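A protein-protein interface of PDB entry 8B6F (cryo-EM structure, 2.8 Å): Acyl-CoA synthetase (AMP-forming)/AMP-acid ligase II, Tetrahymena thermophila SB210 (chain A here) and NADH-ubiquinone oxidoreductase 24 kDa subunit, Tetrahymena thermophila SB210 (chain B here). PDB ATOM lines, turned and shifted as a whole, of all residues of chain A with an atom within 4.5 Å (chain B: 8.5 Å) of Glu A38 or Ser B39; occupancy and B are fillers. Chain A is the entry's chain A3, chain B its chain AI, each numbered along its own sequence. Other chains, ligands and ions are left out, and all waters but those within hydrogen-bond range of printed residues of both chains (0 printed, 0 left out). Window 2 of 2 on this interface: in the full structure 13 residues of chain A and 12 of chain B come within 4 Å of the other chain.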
ATOM      1  N   ARG A  36     -12.998 -22.087 -16.106  1.00  0.00           N
ATOM      2  CA  ARG A  36     -13.422 -22.236 -17.490  1.00  0.00           C
ATOM      3  C   ARG A  36     -12.394 -21.574 -18.392  1.00  0.00           C
ATOM      4  O   ARG A  36     -11.887 -20.493 -18.079  1.00  0.00           O
ATOM      5  CB  ARG A  36     -14.804 -21.608 -17.706  1.00  0.00           C
ATOM      6  CG  ARG A  36     -15.251 -21.477 -19.160  1.00  0.00           C
ATOM      7  CD  ARG A  36     -15.531 -22.823 -19.800  1.00  0.00           C
ATOM      8  NE  ARG A  36     -16.102 -22.671 -21.133  1.00  0.00           N
ATOM      9  CZ  ARG A  36     -16.514 -23.676 -21.894  1.00  0.00           C
ATOM     10  NH1 ARG A  36     -16.434 -24.931 -21.485  1.00  0.00           N
ATOM     11  NH2 ARG A  36     -17.015 -23.415 -23.097  1.00  0.00           N
ATOM     12  N   TYR A  37     -12.093 -22.223 -19.514  1.00  0.00           N
ATOM     13  CA  TYR A  37     -11.164 -21.700 -20.512  1.00  0.00           C
ATOM     14  C   TYR A  37     -11.941 -21.549 -21.816  1.00  0.00           C
ATOM     15  O   TYR A  37     -12.005 -22.474 -22.629  1.00  0.00           O
ATOM     16  CB  TYR A  37      -9.961 -22.615 -20.670  1.00  0.00           C
ATOM     17  CG  TYR A  37      -9.184 -22.801 -19.390  1.00  0.00           C
ATOM     18  CD1 TYR A  37      -8.370 -21.791 -18.897  1.00  0.00           C
ATOM     19  CD2 TYR A  37      -9.263 -23.987 -18.674  1.00  0.00           C
ATOM     20  CE1 TYR A  37      -7.659 -21.956 -17.727  1.00  0.00           C
ATOM     21  CE2 TYR A  37      -8.556 -24.162 -17.503  1.00  0.00           C
ATOM     22  CZ  TYR A  37      -7.756 -23.143 -17.034  1.00  0.00           C
ATOM     23  OH  TYR A  37      -7.047 -23.313 -15.868  1.00  0.00           O
ATOM     24  N   GLU A  38     -12.532 -20.369 -22.007  1.00  0.00           N
ATOM     25  CA  GLU A  38     -13.383 -20.147 -23.169  1.00  0.00           C
ATOM     26  C   GLU A  38     -12.590 -20.232 -24.466  1.00  0.00           C
ATOM     27  O   GLU A  38     -13.082 -20.760 -25.470  1.00  0.00           O
ATOM     28  CB  GLU A  38     -14.070 -18.789 -23.056  1.00  0.00           C
ATOM     29  CG  GLU A  38     -15.115 -18.550 -24.125  1.00  0.00           C
ATOM     30  CD  GLU A  38     -16.285 -19.511 -24.027  1.00  0.00           C
ATOM     31  OE1 GLU A  38     -16.447 -20.147 -22.964  1.00  0.00           O
ATOM     32  OE2 GLU A  38     -17.042 -19.631 -25.012  1.00  0.00           O
ATOM     33  N   ASN A  39     -11.360 -19.715 -24.468  1.00  0.00           N
ATOM     34  CA  ASN A  39     -10.574 -19.695 -25.699  1.00  0.00           C
ATOM     35  C   ASN A  39     -10.336 -21.104 -26.224  1.00  0.00           C
ATOM     36  O   ASN A  39     -10.444 -21.348 -27.432  1.00  0.00           O
ATOM     37  CB  ASN A  39      -9.247 -18.971 -25.466  1.00  0.00           C
ATOM     38  CG  ASN A  39      -8.516 -19.477 -24.241  1.00  0.00           C
ATOM     39  OD1 ASN A  39      -9.011 -20.345 -23.525  1.00  0.00           O
ATOM     40  ND2 ASN A  39      -7.329 -18.936 -23.994  1.00  0.00           N
ATOM     41  N   GLN A  40     -10.009 -22.043 -25.339  1.00  0.00           N
ATOM     42  CA  GLN A  40      -9.776 -23.427 -25.725  1.00  0.00           C
ATOM     43  C   GLN A  40     -10.922 -24.351 -25.333  1.00  0.00           C
ATOM     44  O   GLN A  40     -10.813 -25.566 -25.527  1.00  0.00           O
ATOM     45  CB  GLN A  40      -8.455 -23.935 -25.132  1.00  0.00           C
ATOM     46  CG  GLN A  40      -8.208 -23.562 -23.678  1.00  0.00           C
ATOM     47  CD  GLN A  40      -6.831 -23.984 -23.201  1.00  0.00           C
ATOM     48  OE1 GLN A  40      -6.169 -23.253 -22.465  1.00  0.00           O
ATOM     49  NE2 GLN A  40      -6.392 -25.167 -23.618  1.00  0.00           N
ATOM     50  N   ASN A  41     -12.016 -23.810 -24.795  1.00  0.00           N
ATOM     51  CA  ASN A  41     -13.256 -24.558 -24.585  1.00  0.00           C
ATOM     52  C   ASN A  41     -13.019 -25.817 -23.748  1.00  0.00           C
ATOM     53  O   ASN A  41     -13.206 -26.947 -24.204  1.00  0.00           O
ATOM     54  CB  ASN A  41     -13.899 -24.907 -25.934  1.00  0.00           C
ATOM     55  CG  ASN A  41     -15.299 -25.473 -25.787  1.00  0.00           C
ATOM     56  OD1 ASN A  41     -15.645 -26.057 -24.760  1.00  0.00           O
ATOM     57  ND2 ASN A  41     -16.115 -25.302 -26.820  1.00  0.00           N
ATOM     58  N   TYR A 262     -11.347 -17.665 -18.101  1.00  0.00           N
ATOM     59  CA  TYR A 262     -10.256 -17.038 -18.837  1.00  0.00           C
ATOM     60  C   TYR A 262     -10.611 -16.971 -20.316  1.00  0.00           C
ATOM     61  O   TYR A 262     -10.983 -17.984 -20.917  1.00  0.00           O
ATOM     62  CB  TYR A 262      -8.949 -17.809 -18.645  1.00  0.00           C
ATOM     63  CG  TYR A 262      -8.360 -17.682 -17.259  1.00  0.00           C
ATOM     64  CD1 TYR A 262      -8.744 -18.537 -16.235  1.00  0.00           C
ATOM     65  CD2 TYR A 262      -7.411 -16.709 -16.980  1.00  0.00           C
ATOM     66  CE1 TYR A 262      -8.202 -18.419 -14.969  1.00  0.00           C
ATOM     67  CE2 TYR A 262      -6.863 -16.584 -15.723  1.00  0.00           C
ATOM     68  CZ  TYR A 262      -7.260 -17.441 -14.722  1.00  0.00           C
ATOM     69  OH  TYR A 262      -6.709 -17.307 -13.470  1.00  0.00           O
ATOM     70  N   GLN A 266      -9.078 -13.490 -26.768  1.00  0.00           N
ATOM     71  CA  GLN A 266     -10.367 -13.059 -27.291  1.00  0.00           C
ATOM     72  C   GLN A 266     -10.583 -11.571 -27.034  1.00  0.00           C
ATOM     73  O   GLN A 266     -10.289 -11.059 -25.952  1.00  0.00           O
ATOM     74  CB  GLN A 266     -11.493 -13.872 -26.652  1.00  0.00           C
ATOM     75  CG  GLN A 266     -11.459 -15.350 -27.004  1.00  0.00           C
ATOM     76  CD  GLN A 266     -12.676 -16.091 -26.498  1.00  0.00           C
ATOM     77  OE1 GLN A 266     -13.489 -15.540 -25.759  1.00  0.00           O
ATOM     78  NE2 GLN A 266     -12.807 -17.352 -26.894  1.00  0.00           N
ATOM     79  N   THR A 274     -19.556 -14.520 -24.316  1.00  0.00           N
ATOM     80  CA  THR A 274     -19.430 -15.391 -23.151  1.00  0.00           C
ATOM     81  C   THR A 274     -20.014 -14.701 -21.922  1.00  0.00           C
ATOM     82  O   THR A 274     -20.701 -15.326 -21.106  1.00  0.00           O
ATOM     83  CB  THR A 274     -17.964 -15.742 -22.915  1.00  0.00           C
ATOM     84  OG1 THR A 274     -17.327 -15.975 -24.176  1.00  0.00           O
ATOM     85  CG2 THR A 274     -17.849 -16.982 -22.039  1.00  0.00           C
ATOM     86  N   PHE A 277     -24.103 -14.621 -20.769  1.00  0.00           N
ATOM     87  CA  PHE A 277     -24.721 -15.659 -19.953  1.00  0.00           C
ATOM     88  C   PHE A 277     -24.449 -15.413 -18.475  1.00  0.00           C
ATOM     89  O   PHE A 277     -25.341 -15.571 -17.635  1.00  0.00           O
ATOM     90  CB  PHE A 277     -24.169 -17.024 -20.356  1.00  0.00           C
ATOM     91  CG  PHE A 277     -24.241 -17.307 -21.828  1.00  0.00           C
ATOM     92  CD1 PHE A 277     -25.234 -16.757 -22.620  1.00  0.00           C
ATOM     93  CD2 PHE A 277     -23.287 -18.113 -22.423  1.00  0.00           C
ATOM     94  CE1 PHE A 277     -25.284 -17.030 -23.976  1.00  0.00           C
ATOM     95  CE2 PHE A 277     -23.330 -18.389 -23.771  1.00  0.00           C
ATOM     96  CZ  PHE A 277     -24.326 -17.842 -24.551  1.00  0.00           C
ATOM     97  N   TYR A 278     -23.221 -15.030 -18.141  1.00  0.00           N
ATOM     98  CA  TYR A 278     -22.850 -14.799 -16.753  1.00  0.00           C
ATOM     99  C   TYR A 278     -23.523 -13.519 -16.262  1.00  0.00           C
ATOM    100  O   TYR A 278     -23.693 -12.557 -17.015  1.00  0.00           O
ATOM    101  CB  TYR A 278     -21.328 -14.747 -16.623  1.00  0.00           C
ATOM    102  CG  TYR A 278     -20.709 -16.099 -16.914  1.00  0.00           C
ATOM    103  CD1 TYR A 278     -20.526 -16.523 -18.224  1.00  0.00           C
ATOM    104  CD2 TYR A 278     -20.374 -16.977 -15.888  1.00  0.00           C
ATOM    105  CE1 TYR A 278     -19.993 -17.764 -18.509  1.00  0.00           C
ATOM    106  CE2 TYR A 278     -19.833 -18.225 -16.166  1.00  0.00           C
ATOM    107  CZ  TYR A 278     -19.647 -18.609 -17.480  1.00  0.00           C
ATOM    108  OH  TYR A 278     -19.117 -19.845 -17.776  1.00  0.00           O
ATOM    109  N   ASN B  33     -28.540 -23.350 -31.571  1.00  0.00           N
ATOM    110  CA  ASN B  33     -29.100 -22.160 -30.951  1.00  0.00           C
ATOM    111  C   ASN B  33     -27.994 -21.382 -30.254  1.00  0.00           C
ATOM    112  O   ASN B  33     -27.087 -21.972 -29.661  1.00  0.00           O
ATOM    113  CB  ASN B  33     -30.197 -22.525 -29.947  1.00  0.00           C
ATOM    114  CG  ASN B  33     -30.841 -21.306 -29.320  1.00  0.00           C
ATOM    115  OD1 ASN B  33     -30.668 -20.184 -29.795  1.00  0.00           O
ATOM    116  ND2 ASN B  33     -31.593 -21.523 -28.248  1.00  0.00           N
ATOM    117  N   ASP B  34     -28.072 -20.052 -30.335  1.00  0.00           N
ATOM    118  CA  ASP B  34     -27.045 -19.219 -29.720  1.00  0.00           C
ATOM    119  C   ASP B  34     -27.152 -19.219 -28.202  1.00  0.00           C
ATOM    120  O   ASP B  34     -26.145 -19.024 -27.511  1.00  0.00           O
ATOM    121  CB  ASP B  34     -27.143 -17.788 -30.252  1.00  0.00           C
ATOM    122  CG  ASP B  34     -27.016 -17.719 -31.761  1.00  0.00           C
ATOM    123  OD1 ASP B  34     -26.914 -18.787 -32.400  1.00  0.00           O
ATOM    124  OD2 ASP B  34     -27.014 -16.596 -32.308  1.00  0.00           O
ATOM    125  N   ASP B  35     -28.351 -19.433 -27.665  1.00  0.00           N
ATOM    126  CA  ASP B  35     -28.567 -19.440 -26.226  1.00  0.00           C
ATOM    127  C   ASP B  35     -28.407 -20.824 -25.613  1.00  0.00           C
ATOM    128  O   ASP B  35     -28.611 -20.976 -24.404  1.00  0.00           O
ATOM    129  CB  ASP B  35     -29.961 -18.896 -25.900  1.00  0.00           C
ATOM    130  CG  ASP B  35     -30.124 -17.441 -26.287  1.00  0.00           C
ATOM    131  OD1 ASP B  35     -29.145 -16.847 -26.785  1.00  0.00           O
ATOM    132  OD2 ASP B  35     -31.227 -16.890 -26.094  1.00  0.00           O
ATOM    133  N   ASN B  36     -28.055 -21.831 -26.411  1.00  0.00           N
ATOM    134  CA  ASN B  36     -27.822 -23.181 -25.914  1.00  0.00           C
ATOM    135  C   ASN B  36     -26.458 -23.690 -26.360  1.00  0.00           C
ATOM    136  O   ASN B  36     -26.248 -24.899 -26.489  1.00  0.00           O
ATOM    137  CB  ASN B  36     -28.928 -24.129 -26.377  1.00  0.00           C
ATOM    138  CG  ASN B  36     -28.892 -25.459 -25.657  1.00  0.00           C
ATOM    139  OD1 ASN B  36     -28.346 -25.568 -24.562  1.00  0.00           O
ATOM    140  ND2 ASN B  36     -29.478 -26.480 -26.270  1.00  0.00           N
ATOM    141  N   SER B  37     -25.520 -22.779 -26.600  1.00  0.00           N
ATOM    142  CA  SER B  37     -24.186 -23.169 -27.018  1.00  0.00           C
ATOM    143  C   SER B  37     -23.431 -23.802 -25.851  1.00  0.00           C
ATOM    144  O   SER B  37     -23.856 -23.753 -24.694  1.00  0.00           O
ATOM    145  CB  SER B  37     -23.418 -21.964 -27.560  1.00  0.00           C
ATOM    146  OG  SER B  37     -23.285 -20.954 -26.574  1.00  0.00           O
ATOM    147  N   ASP B  38     -22.286 -24.405 -26.173  1.00  0.00           N
ATOM    148  CA  ASP B  38     -21.466 -25.029 -25.142  1.00  0.00           C
ATOM    149  C   ASP B  38     -20.967 -24.004 -24.132  1.00  0.00           C
ATOM    150  O   ASP B  38     -20.679 -24.354 -22.983  1.00  0.00           O
ATOM    151  CB  ASP B  38     -20.288 -25.758 -25.787  1.00  0.00           C
ATOM    152  CG  ASP B  38     -19.508 -26.597 -24.796  1.00  0.00           C
ATOM    153  OD1 ASP B  38     -19.966 -26.738 -23.643  1.00  0.00           O
ATOM    154  OD2 ASP B  38     -18.436 -27.118 -25.172  1.00  0.00           O
ATOM    155  N   SER B  39     -20.858 -22.740 -24.539  1.00  0.00           N
ATOM    156  CA  SER B  39     -20.373 -21.693 -23.650  1.00  0.00           C
ATOM    157  C   SER B  39     -21.372 -21.329 -22.560  1.00  0.00           C
ATOM    158  O   SER B  39     -20.998 -20.628 -21.613  1.00  0.00           O
ATOM    159  CB  SER B  39     -20.022 -20.447 -24.464  1.00  0.00           C
ATOM    160  OG  SER B  39     -19.538 -19.410 -23.629  1.00  0.00           O
ATOM    161  N   VAL B  40     -22.619 -21.769 -22.667  1.00  0.00           N
ATOM    162  CA  VAL B  40     -23.616 -21.438 -21.643  1.00  0.00           C
ATOM    163  C   VAL B  40     -23.235 -22.130 -20.337  1.00  0.00           C
ATOM    164  O   VAL B  40     -23.035 -23.356 -20.327  1.00  0.00           O
ATOM    165  CB  VAL B  40     -25.013 -21.858 -22.102  1.00  0.00           C
ATOM    166  CG1 VAL B  40     -26.053 -21.494 -21.052  1.00  0.00           C
ATOM    167  CG2 VAL B  40     -25.356 -21.209 -23.436  1.00  0.00           C
ATOM    168  N   PRO B  41     -23.122 -21.409 -19.224  1.00  0.00           N
ATOM    169  CA  PRO B  41     -22.744 -22.052 -17.963  1.00  0.00           C
ATOM    170  C   PRO B  41     -23.925 -22.735 -17.292  1.00  0.00           C
ATOM    171  O   PRO B  41     -25.091 -22.480 -17.596  1.00  0.00           O
ATOM    172  CB  PRO B  41     -22.237 -20.883 -17.115  1.00  0.00           C
ATOM    173  CG  PRO B  41     -23.031 -19.725 -17.592  1.00  0.00           C
ATOM    174  CD  PRO B  41     -23.269 -19.951 -19.066  1.00  0.00           C
ATOM    175  N   PHE B  42     -23.592 -23.622 -16.359  1.00  0.00           N
ATOM    176  CA  PHE B  42     -24.600 -24.276 -15.535  1.00  0.00           C
ATOM    177  C   PHE B  42     -23.919 -24.858 -14.308  1.00  0.00           C
ATOM    178  O   PHE B  42     -22.924 -25.578 -14.435  1.00  0.00           O
ATOM    179  CB  PHE B  42     -25.332 -25.374 -16.307  1.00  0.00           C
ATOM    180  CG  PHE B  42     -26.342 -26.105 -15.480  1.00  0.00           C
ATOM    181  CD1 PHE B  42     -27.610 -25.581 -15.299  1.00  0.00           C
ATOM    182  CD2 PHE B  42     -26.022 -27.305 -14.870  1.00  0.00           C
ATOM    183  CE1 PHE B  42     -28.542 -26.243 -14.534  1.00  0.00           C
ATOM    184  CE2 PHE B  42     -26.950 -27.971 -14.102  1.00  0.00           C
ATOM    185  CZ  PHE B  42     -28.212 -27.437 -13.934  1.00  0.00           C
ATOM    186  N   LEU B  85     -27.477 -28.000 -22.844  1.00  0.00           N
ATOM    187  CA  LEU B  85     -26.431 -28.947 -23.220  1.00  0.00           C
ATOM    188  C   LEU B  85     -25.280 -28.922 -22.224  1.00  0.00           C
ATOM    189  O   LEU B  85     -24.706 -29.967 -21.900  1.00  0.00           O
ATOM    190  CB  LEU B  85     -25.928 -28.638 -24.630  1.00  0.00           C
ATOM    191  CG  LEU B  85     -24.860 -29.584 -25.184  1.00  0.00           C
ATOM    192  CD1 LEU B  85     -25.393 -31.001 -25.312  1.00  0.00           C
ATOM    193  CD2 LEU B  85     -24.356 -29.082 -26.526  1.00  0.00           C
ATOM    194  N   SER B  86     -24.926 -27.736 -21.728  1.00  0.00           N
ATOM    195  CA  SER B  86     -23.896 -27.644 -20.699  1.00  0.00           C
ATOM    196  C   SER B  86     -24.312 -28.399 -19.443  1.00  0.00           C
ATOM    197  O   SER B  86     -23.491 -29.082 -18.820  1.00  0.00           O
ATOM    198  CB  SER B  86     -23.606 -26.180 -20.377  1.00  0.00           C
ATOM    199  OG  SER B  86     -24.774 -25.510 -19.936  1.00  0.00           O
ATOM    200  N   LYS B  89     -23.816 -32.087 -20.068  1.00  0.00           N
ATOM    201  CA  LYS B  89     -22.405 -32.442 -19.951  1.00  0.00           C
ATOM    202  C   LYS B  89     -21.966 -32.475 -18.492  1.00  0.00           C
ATOM    203  O   LYS B  89     -21.205 -33.359 -18.084  1.00  0.00           O
ATOM    204  CB  LYS B  89     -21.546 -31.461 -20.750  1.00  0.00           C
ATOM    205  CG  LYS B  89     -21.766 -31.547 -22.249  1.00  0.00           C
ATOM    206  CD  LYS B  89     -20.844 -30.607 -23.004  1.00  0.00           C
ATOM    207  CE  LYS B  89     -21.036 -30.753 -24.505  1.00  0.00           C
ATOM    208  NZ  LYS B  89     -20.123 -29.866 -25.273  1.00  0.00           N
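The side-chain amide oxygen (OD1) of Asn A41 sits close to the side-chain carboxylate (OD2) of Asp B38 (3.0 Å). OG of Ser B39 lies within hydrogen-bond range of OE2 of Glu A38, 2.9 Å away.
Arg A36 touches Asp B38 (NH2 to O, 3.8 Å). NH2 of Arg A36 touches CA of Ser B39, at 3.8 Å. Thr A274 touches Ser B39. Asp B34 touches Phe A277. CE2 of Phe A277 touches OG of Ser B37, 3.8 Å away. Ser B39 touches Phe A277 (O to CD2, 3.5 Å). Phe A277 touches Val B40. Phe A277 touches Pro B41. Tyr A278 touches Pro B41 (OH to CB, 3.4 Å).
Of the printed residues of chain B, Arg A36 touches Asp B38 (3.8 Å) and Ser B39 (3.8 Å). Glu A38 touches just one residue of chain B: Ser B39 (2.9 Å). Asn A39 touches none of the printed residues of chain B. Printed residues of chain B within 4 Å of Thr A274: Ser B39. Of the printed residues of chain B, Phe A277 touches Asp B34 (3.7 Å), Ser B37 (3.8 Å), Ser B39 (3.5 Å), Val B40 (3.4 Å) and Pro B41 (3.3 Å). Ser B39 touches just these residues of chain A: Arg A36, Glu A38, Thr A274 and Phe A277. Lys B89 touches none of the printed residues of chain A. The nearest residue of chain B that does not touch Glu A38 is Asp B38 (5.9 Å). The nearest residue of chain A that does not touch Ser B39 is Tyr A278 (4.3 Å). The nearest printed residue of chain A that does not touch Asp B34 is Thr A274 (8.6 Å).
Of the 11 printed residues of chain A, 6 touch a printed residue of chain B. Printed residues of chain A that touch a printed residue of chain B: Arg A36, Glu A38, Asn A41, Thr A274, Phe A277 and Tyr A278. Hydrophobic or aromatic side chains of chain A that line the printed part of chain B: Phe A277 and Tyr A278. Printed residues of chain B that touch a printed residue of chain A: Asp B34, Ser B37, Asp B38, Ser B39, Val B40 and Pro B41. Hydrophobic or aromatic side chains of chain B within 4 Å of the printed part of chain A: Val B40 and Pro B41. Among the printed residues, 11 pairs touch across the chains.
The side-chain amino group of Lys B89 lies within salt-bridge range of the side-chain carboxylate of Asp B38. O of Val B40 lies within hydrogen-bond range of OG of Ser B86, at 2.8 Å. The guanidinium group of Arg A36 is in salt-bridge range of the side-chain carboxylate of Glu A38, 3.1 Å away. NH2 of Arg A36 lies within hydrogen-bond range of OD1 of Asn A41 (3.4 Å). O of Arg A36 lies within hydrogen-bond range of N of Tyr A262 (2.9 Å). O of Tyr A262 sits at hydrogen-bond distance from N of Glu A38 (3.0 Å).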
